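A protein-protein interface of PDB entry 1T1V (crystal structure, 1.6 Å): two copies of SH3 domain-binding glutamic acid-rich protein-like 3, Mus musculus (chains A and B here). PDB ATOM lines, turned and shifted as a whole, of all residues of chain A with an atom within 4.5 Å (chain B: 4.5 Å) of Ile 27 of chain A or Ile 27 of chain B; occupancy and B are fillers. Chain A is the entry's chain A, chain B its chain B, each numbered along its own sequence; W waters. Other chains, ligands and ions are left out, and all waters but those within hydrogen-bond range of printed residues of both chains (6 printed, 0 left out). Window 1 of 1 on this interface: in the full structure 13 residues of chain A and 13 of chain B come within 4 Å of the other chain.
NZ of Lys 31 of chain A is in hydrogen-bond range of O of Gly 30 of chain B (2.7 Å).
The guanidinium group (NH1) of Arg 26 of chain B is in salt-bridge range of the side-chain carboxylate (OE2) of Glu 23 of chain A, 3.0 Å away.
The backbone carbonyl oxygen (O) of Gly 30 of chain A lies within hydrogen-bond range of the side-chain amino group (NZ) of Lys 31 of chain B, at 2.6 Å.
Among the printed residues, pairs that only touch across the chains: Glu 23 of chain A with Glu 23 of chain B (3.6 Å), Arg 26 of chain A with Glu 23 of chain B (3.7 Å), Arg 26 of chain A with Ile 27 of chain B (3.9 Å), Arg 26 of chain A with Val 81 of chain B (3.6 Å), Ile 27 of chain A with Ile 27 of chain B (3.8 Å), Gly 30 of chain A with Val 81 of chain B (3.9 Å), Val 81 of chain A with Arg 26 of chain B (3.6 Å) and Val 81 of chain A with Gly 30 of chain B (3.7 Å).
Ile 27 of chain A touches one residue of chain B.
Ile 27 of chain B touches just these residues of chain A: Arg 26 (3.9 Å) and Ile 27 (3.8 Å).
Of the printed residues of chain B, Val 81 of chain A touches Arg 26 (3.6 Å) and Gly 30 (3.7 Å).
Of the printed residues of chain A, Val 81 of chain B touches Arg 26 (3.6 Å) and Gly 30 (3.9 Å).
Of the printed residues of chain A, Glu 23 of chain B touches Glu 23 and Arg 26.
Leu 28 of chain B touches none of the printed residues of chain A.
The nearest printed residue of chain A that does not touch Ile 27 of chain B is Gly 30 of chain A (4.9 Å).
The nearest printed residue of chain B that does not touch Glu 23 of chain A is Ile 27 of chain B (5.3 Å).
Of the 11 printed residues of chain B, 6 touch a printed residue of chain A.
Among the printed residues, 11 pairs touch across the chains.
Among the printed residues, Asp or Glu carboxylates within 4 Å of a Lys or Arg side-chain nitrogen of the other chain: Glu 23 of chain A with Arg 26 of chain B (3.0 Å).
Glu 23 of chain A touches Arg 26 of chain B, and with the chains exchanged Arg 26 of chain A touches Glu 23 of chain B.
Arg 26 of chain A touches Ile 27 of chain B, but with the chains exchanged Ile 27 of chain A does not touch Arg 26 of chain B (4.3 Å).
Gly 30 of chain A touches Lys 31 of chain B, and with the chains exchanged Lys 31 of chain A touches Gly 30 of chain B.
Gly 30 of chain A touches Val 81 of chain B, and with the chains exchanged Val 81 of chain A touches Gly 30 of chain B.
Positions printed for both chains: 23, 24, 25, 26, 27, 28, 29, 30, 31, 77 and 81.
Of the 11 pairs that touch across the chains among the printed residues, 10 have their exchanged pair printed and touching as well.
Water W4 lies within hydrogen-bond range of OE2 of Glu 23 of chain B and NE of Arg 26 of chain A.
Water W2 bridges the backbone carbonyl oxygen (O) of Val 81 of chain B (2.7 Å) and the backbone carbonyl oxygen (O) of Asp 29 of chain A (3.1 Å).
Water W3 bridges O of Val 81 of chain A (2.7 Å) and O of Asp 29 of chain B (3.0 Å).
Water W6 lies within hydrogen-bond range of NZ of Lys 31 of chain B (2.9 Å) and O of Gly 30 of chain A (3.4 Å).
Water W1 lies within hydrogen-bond range of the backbone carbonyl oxygen (O) of Ile 27 of chain A (3.0 Å) and the backbone carbonyl oxygen (O) of Ile 27 of chain B (3.1 Å).
Water W5 bridges NZ of Lys 31 of chain A (3.1 Å) and O of Gly 30 of chain B (3.5 Å).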
ATOM      1  N   GLU A  23      17.394 -29.887  -1.075  1.00  0.00           N
ATOM      2  CA  GLU A  23      18.776 -29.604  -1.467  1.00  0.00           C
ATOM      3  C   GLU A  23      18.876 -28.280  -2.249  1.00  0.00           C
ATOM      4  O   GLU A  23      19.739 -27.424  -1.955  1.00  0.00           O
ATOM      5  CB  GLU A  23      19.340 -30.739  -2.247  1.00  0.00           C
ATOM      6  CG  GLU A  23      20.864 -30.686  -2.396  1.00  0.00           C
ATOM      7  CD  GLU A  23      21.435 -31.918  -3.079  1.00  0.00           C
ATOM      8  OE1 GLU A  23      21.332 -33.035  -2.553  1.00  0.00           O
ATOM      9  OE2 GLU A  23      21.955 -31.775  -4.182  1.00  0.00           O
ATOM     10  N   VAL A  24      17.997 -28.098  -3.235  1.00  0.00           N
ATOM     11  CA  VAL A  24      17.954 -26.819  -3.968  1.00  0.00           C
ATOM     12  C   VAL A  24      17.845 -25.644  -3.017  1.00  0.00           C
ATOM     13  O   VAL A  24      18.607 -24.693  -3.064  1.00  0.00           O
ATOM     14  CB  VAL A  24      16.829 -26.796  -5.027  1.00  0.00           C
ATOM     15  CG1 VAL A  24      16.565 -25.397  -5.497  1.00  0.00           C
ATOM     16  CG2 VAL A  24      17.108 -27.709  -6.122  1.00  0.00           C
ATOM     17  N   THR A  25      16.827 -25.621  -2.167  1.00  0.00           N
ATOM     18  CA  THR A  25      16.641 -24.484  -1.342  1.00  0.00           C
ATOM     19  C   THR A  25      17.721 -24.254  -0.265  1.00  0.00           C
ATOM     20  O   THR A  25      17.953 -23.126   0.101  1.00  0.00           O
ATOM     21  CB  THR A  25      15.193 -24.506  -0.754  1.00  0.00           C
ATOM     22  OG1 THR A  25      15.025 -25.679   0.061  1.00  0.00           O
ATOM     23  CG2 THR A  25      14.192 -24.488  -1.881  1.00  0.00           C
ATOM     24  N   ARG A  26      18.304 -25.312   0.291  1.00  0.00           N
ATOM     25  CA  ARG A  26      19.360 -25.218   1.289  1.00  0.00           C
ATOM     26  C   ARG A  26      20.623 -24.672   0.612  1.00  0.00           C
ATOM     27  O   ARG A  26      21.386 -23.919   1.219  1.00  0.00           O
ATOM     28  CB  ARG A  26      19.672 -26.587   1.901  1.00  0.00           C
ATOM     29  CG  ARG A  26      19.039 -26.818   3.253  1.00  0.00           C
ATOM     30  CD  ARG A  26      17.582 -27.211   3.158  1.00  0.00           C
ATOM     31  NE  ARG A  26      17.127 -27.844   4.405  1.00  0.00           N
ATOM     32  CZ  ARG A  26      16.360 -27.235   5.326  1.00  0.00           C
ATOM     33  NH1 ARG A  26      15.966 -25.975   5.132  1.00  0.00           N
ATOM     34  NH2 ARG A  26      16.009 -27.896   6.427  1.00  0.00           N
ATOM     35  N   ILE A  27      20.824 -25.064  -0.643  1.00  0.00           N
ATOM     36  CA  ILE A  27      21.974 -24.507  -1.365  1.00  0.00           C
ATOM     37  C   ILE A  27      21.765 -22.985  -1.627  1.00  0.00           C
ATOM     38  O   ILE A  27      22.681 -22.179  -1.426  1.00  0.00           O
ATOM     39  CB  ILE A  27      22.241 -25.257  -2.645  1.00  0.00           C
ATOM     40  CG1 ILE A  27      22.781 -26.650  -2.348  1.00  0.00           C
ATOM     41  CG2 ILE A  27      23.226 -24.506  -3.515  1.00  0.00           C
ATOM     42  CD1 ILE A  27      22.308 -27.701  -3.330  1.00  0.00           C
ATOM     43  N   LEU A  28      20.562 -22.588  -2.069  1.00  0.00           N
ATOM     44  CA  LEU A  28      20.239 -21.191  -2.266  1.00  0.00           C
ATOM     45  C   LEU A  28      20.364 -20.396  -0.948  1.00  0.00           C
ATOM     46  O   LEU A  28      20.861 -19.280  -0.908  1.00  0.00           O
ATOM     47  CB  LEU A  28      18.822 -21.053  -2.839  1.00  0.00           C
ATOM     48  CG  LEU A  28      18.616 -21.507  -4.305  1.00  0.00           C
ATOM     49  CD1 LEU A  28      17.267 -21.252  -4.783  1.00  0.00           C
ATOM     50  CD2 LEU A  28      19.586 -20.785  -5.257  1.00  0.00           C
ATOM     51  N   ASP A  29      19.888 -20.965   0.149  1.00  0.00           N
ATOM     52  CA  ASP A  29      19.953 -20.323   1.461  1.00  0.00           C
ATOM     53  C   ASP A  29      21.403 -20.150   1.931  1.00  0.00           C
ATOM     54  O   ASP A  29      21.712 -19.114   2.510  1.00  0.00           O
ATOM     55  CB  ASP A  29      19.218 -21.153   2.489  1.00  0.00           C
ATOM     56  CG  ASP A  29      17.755 -21.147   2.284  1.00  0.00           C
ATOM     57  OD1 ASP A  29      17.252 -20.416   1.438  1.00  0.00           O
ATOM     58  OD2 ASP A  29      16.979 -21.857   2.962  1.00  0.00           O
ATOM     59  N   GLY A  30      22.232 -21.150   1.686  1.00  0.00           N
ATOM     60  CA  GLY A  30      23.689 -21.121   1.930  1.00  0.00           C
ATOM     61  C   GLY A  30      24.353 -19.955   1.243  1.00  0.00           C
ATOM     62  O   GLY A  30      25.298 -19.351   1.811  1.00  0.00           O
ATOM     63  N   LYS A  31      23.906 -19.641   0.032  1.00  0.00           N
ATOM     64  CA  LYS A  31      24.484 -18.561  -0.760  1.00  0.00           C
ATOM     65  C   LYS A  31      23.790 -17.232  -0.550  1.00  0.00           C
ATOM     66  O   LYS A  31      24.176 -16.235  -1.185  1.00  0.00           O
ATOM     67  CB  LYS A  31      24.463 -18.937  -2.231  1.00  0.00           C
ATOM     68  CG  LYS A  31      25.384 -20.094  -2.581  1.00  0.00           C
ATOM     69  CD  LYS A  31      25.307 -20.498  -4.033  1.00  0.00           C
ATOM     70  CE  LYS A  31      25.976 -19.421  -4.898  1.00  0.00           C
ATOM     71  NZ  LYS A  31      27.444 -19.615  -5.159  1.00  0.00           N
ATOM     72  N   PHE A  77      20.428 -27.851 -11.944  1.00  0.00           N
ATOM     73  CA  PHE A  77      20.866 -27.041 -10.777  1.00  0.00           C
ATOM     74  C   PHE A  77      22.138 -27.633 -10.133  1.00  0.00           C
ATOM     75  O   PHE A  77      23.134 -26.912  -9.971  1.00  0.00           O
ATOM     76  CB  PHE A  77      19.705 -26.869  -9.805  1.00  0.00           C
ATOM     77  CG  PHE A  77      20.040 -26.067  -8.580  1.00  0.00           C
ATOM     78  CD1 PHE A  77      20.660 -26.629  -7.458  1.00  0.00           C
ATOM     79  CD2 PHE A  77      19.705 -24.741  -8.517  1.00  0.00           C
ATOM     80  CE1 PHE A  77      20.933 -25.856  -6.299  1.00  0.00           C
ATOM     81  CE2 PHE A  77      19.966 -23.988  -7.380  1.00  0.00           C
ATOM     82  CZ  PHE A  77      20.577 -24.552  -6.285  1.00  0.00           C
ATOM     83  N   VAL A  81      25.992 -25.989  -9.806  1.00  0.00           N
ATOM     84  CA  VAL A  81      26.761 -25.946  -8.578  1.00  0.00           C
ATOM     85  C   VAL A  81      28.104 -26.622  -8.773  1.00  0.00           C
ATOM     86  O   VAL A  81      29.136 -26.043  -8.444  1.00  0.00           O
ATOM     87  CB  VAL A  81      26.037 -26.582  -7.404  1.00  0.00           C
ATOM     88  CG1 VAL A  81      26.877 -26.512  -6.113  1.00  0.00           C
ATOM     89  CG2 VAL A  81      24.730 -25.850  -7.163  1.00  0.00           C
ATOM     90  N   GLU B  23      24.165 -33.571   0.056  1.00  0.00           N
ATOM     91  CA  GLU B  23      23.704 -32.263   0.424  1.00  0.00           C
ATOM     92  C   GLU B  23      24.806 -31.448   1.121  1.00  0.00           C
ATOM     93  O   GLU B  23      24.964 -30.307   0.779  1.00  0.00           O
ATOM     94  CB  GLU B  23      22.413 -32.273   1.261  1.00  0.00           C
ATOM     95  CG  GLU B  23      21.917 -30.878   1.523  1.00  0.00           C
ATOM     96  CD  GLU B  23      20.464 -30.928   2.024  1.00  0.00           C
ATOM     97  OE1 GLU B  23      19.632 -31.585   1.400  1.00  0.00           O
ATOM     98  OE2 GLU B  23      20.180 -30.365   3.070  1.00  0.00           O
ATOM     99  N   VAL B  24      25.559 -32.051   2.026  1.00  0.00           N
ATOM    100  CA  VAL B  24      26.557 -31.358   2.785  1.00  0.00           C
ATOM    101  C   VAL B  24      27.618 -30.948   1.787  1.00  0.00           C
ATOM    102  O   VAL B  24      28.007 -29.737   1.738  1.00  0.00           O
ATOM    103  CB  VAL B  24      27.164 -32.232   3.909  1.00  0.00           C
ATOM    104  CG1 VAL B  24      28.469 -31.658   4.416  1.00  0.00           C
ATOM    105  CG2 VAL B  24      26.192 -32.243   5.060  1.00  0.00           C
ATOM    106  N   THR B  25      28.046 -31.891   0.985  1.00  0.00           N
ATOM    107  CA  THR B  25      29.208 -31.511   0.112  1.00  0.00           C
ATOM    108  C   THR B  25      28.774 -30.479  -0.964  1.00  0.00           C
ATOM    109  O   THR B  25      29.587 -29.606  -1.354  1.00  0.00           O
ATOM    110  CB  THR B  25      29.877 -32.716  -0.553  1.00  0.00           C
ATOM    111  OG1 THR B  25      28.919 -33.427  -1.356  1.00  0.00           O
ATOM    112  CG2 THR B  25      30.500 -33.617   0.462  1.00  0.00           C
ATOM    113  N   ARG B  26      27.553 -30.564  -1.476  1.00  0.00           N
ATOM    114  CA  ARG B  26      27.029 -29.621  -2.495  1.00  0.00           C
ATOM    115  C   ARG B  26      26.824 -28.288  -1.888  1.00  0.00           C
ATOM    116  O   ARG B  26      27.026 -27.293  -2.597  1.00  0.00           O
ATOM    117  CB  ARG B  26      25.782 -30.173  -3.175  1.00  0.00           C
ATOM    118  CG  ARG B  26      26.171 -31.313  -4.053  1.00  0.00           C
ATOM    119  CD  ARG B  26      25.072 -31.938  -4.793  1.00  0.00           C
ATOM    120  NE  ARG B  26      25.486 -33.150  -5.519  1.00  0.00           N
ATOM    121  CZ  ARG B  26      24.635 -34.120  -5.884  1.00  0.00           C
ATOM    122  NH1 ARG B  26      23.351 -34.042  -5.586  1.00  0.00           N
ATOM    123  NH2 ARG B  26      25.084 -35.200  -6.513  1.00  0.00           N
ATOM    124  N   ILE B  27      26.384 -28.189  -0.622  1.00  0.00           N
ATOM    125  CA  ILE B  27      26.238 -26.874   0.026  1.00  0.00           C
ATOM    126  C   ILE B  27      27.631 -26.210   0.096  1.00  0.00           C
ATOM    127  O   ILE B  27      27.742 -25.017  -0.230  1.00  0.00           O
ATOM    128  CB  ILE B  27      25.541 -26.936   1.386  1.00  0.00           C
ATOM    129  CG1 ILE B  27      24.074 -27.294   1.149  1.00  0.00           C
ATOM    130  CG2 ILE B  27      25.691 -25.613   2.124  1.00  0.00           C
ATOM    131  CD1 ILE B  27      23.380 -27.805   2.317  1.00  0.00           C
ATOM    132  N   LEU B  28      28.613 -26.970   0.549  1.00  0.00           N
ATOM    133  CA  LEU B  28      30.001 -26.465   0.631  1.00  0.00           C
ATOM    134  C   LEU B  28      30.489 -26.079  -0.714  1.00  0.00           C
ATOM    135  O   LEU B  28      31.141 -25.007  -0.855  1.00  0.00           O
ATOM    136  CB  LEU B  28      30.908 -27.477   1.323  1.00  0.00           C
ATOM    137  CG  LEU B  28      30.682 -27.749   2.815  1.00  0.00           C
ATOM    138  CD1 LEU B  28      31.627 -28.856   3.349  1.00  0.00           C
ATOM    139  CD2 LEU B  28      30.779 -26.510   3.676  1.00  0.00           C
ATOM    140  N   ASP B  29      30.255 -26.895  -1.729  1.00  0.00           N
ATOM    141  CA  ASP B  29      30.629 -26.533  -3.106  1.00  0.00           C
ATOM    142  C   ASP B  29      29.957 -25.239  -3.582  1.00  0.00           C
ATOM    143  O   ASP B  29      30.598 -24.398  -4.208  1.00  0.00           O
ATOM    144  CB  ASP B  29      30.353 -27.632  -4.111  1.00  0.00           C
ATOM    145  CG  ASP B  29      31.082 -28.923  -3.812  1.00  0.00           C
ATOM    146  OD1 ASP B  29      32.079 -28.943  -3.063  1.00  0.00           O
ATOM    147  OD2 ASP B  29      30.693 -30.018  -4.261  1.00  0.00           O
ATOM    148  N   GLY B  30      28.671 -25.065  -3.277  1.00  0.00           N
ATOM    149  CA  GLY B  30      27.932 -23.861  -3.593  1.00  0.00           C
ATOM    150  C   GLY B  30      28.548 -22.634  -2.933  1.00  0.00           C
ATOM    151  O   GLY B  30      28.521 -21.586  -3.575  1.00  0.00           O
ATOM    152  N   LYS B  31      29.108 -22.740  -1.745  1.00  0.00           N
ATOM    153  CA  LYS B  31      29.676 -21.599  -1.026  1.00  0.00           C
ATOM    154  C   LYS B  31      31.158 -21.449  -1.388  1.00  0.00           C
ATOM    155  O   LYS B  31      31.810 -20.528  -0.914  1.00  0.00           O
ATOM    156  CB  LYS B  31      29.484 -21.752   0.438  1.00  0.00           C
ATOM    157  CG  LYS B  31      27.989 -21.611   0.827  1.00  0.00           C
ATOM    158  CD  LYS B  31      27.812 -21.706   2.306  1.00  0.00           C
ATOM    159  CE  LYS B  31      28.403 -20.542   3.125  1.00  0.00           C
ATOM    160  NZ  LYS B  31      27.655 -19.279   3.006  1.00  0.00           N
ATOM    161  N   PHE B  77      24.780 -29.237  10.789  1.00  0.00           N
ATOM    162  CA  PHE B  77      25.215 -28.544   9.584  1.00  0.00           C
ATOM    163  C   PHE B  77      24.057 -27.811   8.916  1.00  0.00           C
ATOM    164  O   PHE B  77      24.116 -26.614   8.649  1.00  0.00           O
ATOM    165  CB  PHE B  77      25.845 -29.534   8.593  1.00  0.00           C
ATOM    166  CG  PHE B  77      26.293 -28.908   7.327  1.00  0.00           C
ATOM    167  CD1 PHE B  77      25.474 -28.691   6.235  1.00  0.00           C
ATOM    168  CD2 PHE B  77      27.625 -28.548   7.207  1.00  0.00           C
ATOM    169  CE1 PHE B  77      25.936 -28.130   5.097  1.00  0.00           C
ATOM    170  CE2 PHE B  77      28.079 -27.949   6.020  1.00  0.00           C
ATOM    171  CZ  PHE B  77      27.264 -27.757   4.986  1.00  0.00           C
ATOM    172  N   VAL B  81      23.446 -23.725   8.225  1.00  0.00           N
ATOM    173  CA  VAL B  81      23.109 -23.171   6.936  1.00  0.00           C
ATOM    174  C   VAL B  81      21.877 -22.282   7.093  1.00  0.00           C
ATOM    175  O   VAL B  81      21.820 -21.150   6.685  1.00  0.00           O
ATOM    176  CB  VAL B  81      22.894 -24.223   5.879  1.00  0.00           C
ATOM    177  CG1 VAL B  81      22.289 -23.656   4.654  1.00  0.00           C
ATOM    178  CG2 VAL B  81      24.153 -25.070   5.663  1.00  0.00           C
HETATM  179  O   HOH W   1      25.472 -23.055  -0.808  1.00  0.00           O
HETATM  180  O   HOH W   2      23.189 -19.330   5.270  1.00  0.00           O
HETATM  181  O   HOH W   3      29.496 -23.820  -6.893  1.00  0.00           O
HETATM  182  O   HOH W   4      17.880 -30.664   4.257  1.00  0.00           O
HETATM  183  O   HOH W   5      27.329 -22.286  -6.752  1.00  0.00           O
HETATM  184  O   HOH W   6      25.757 -20.077   5.086  1.00  0.00           O
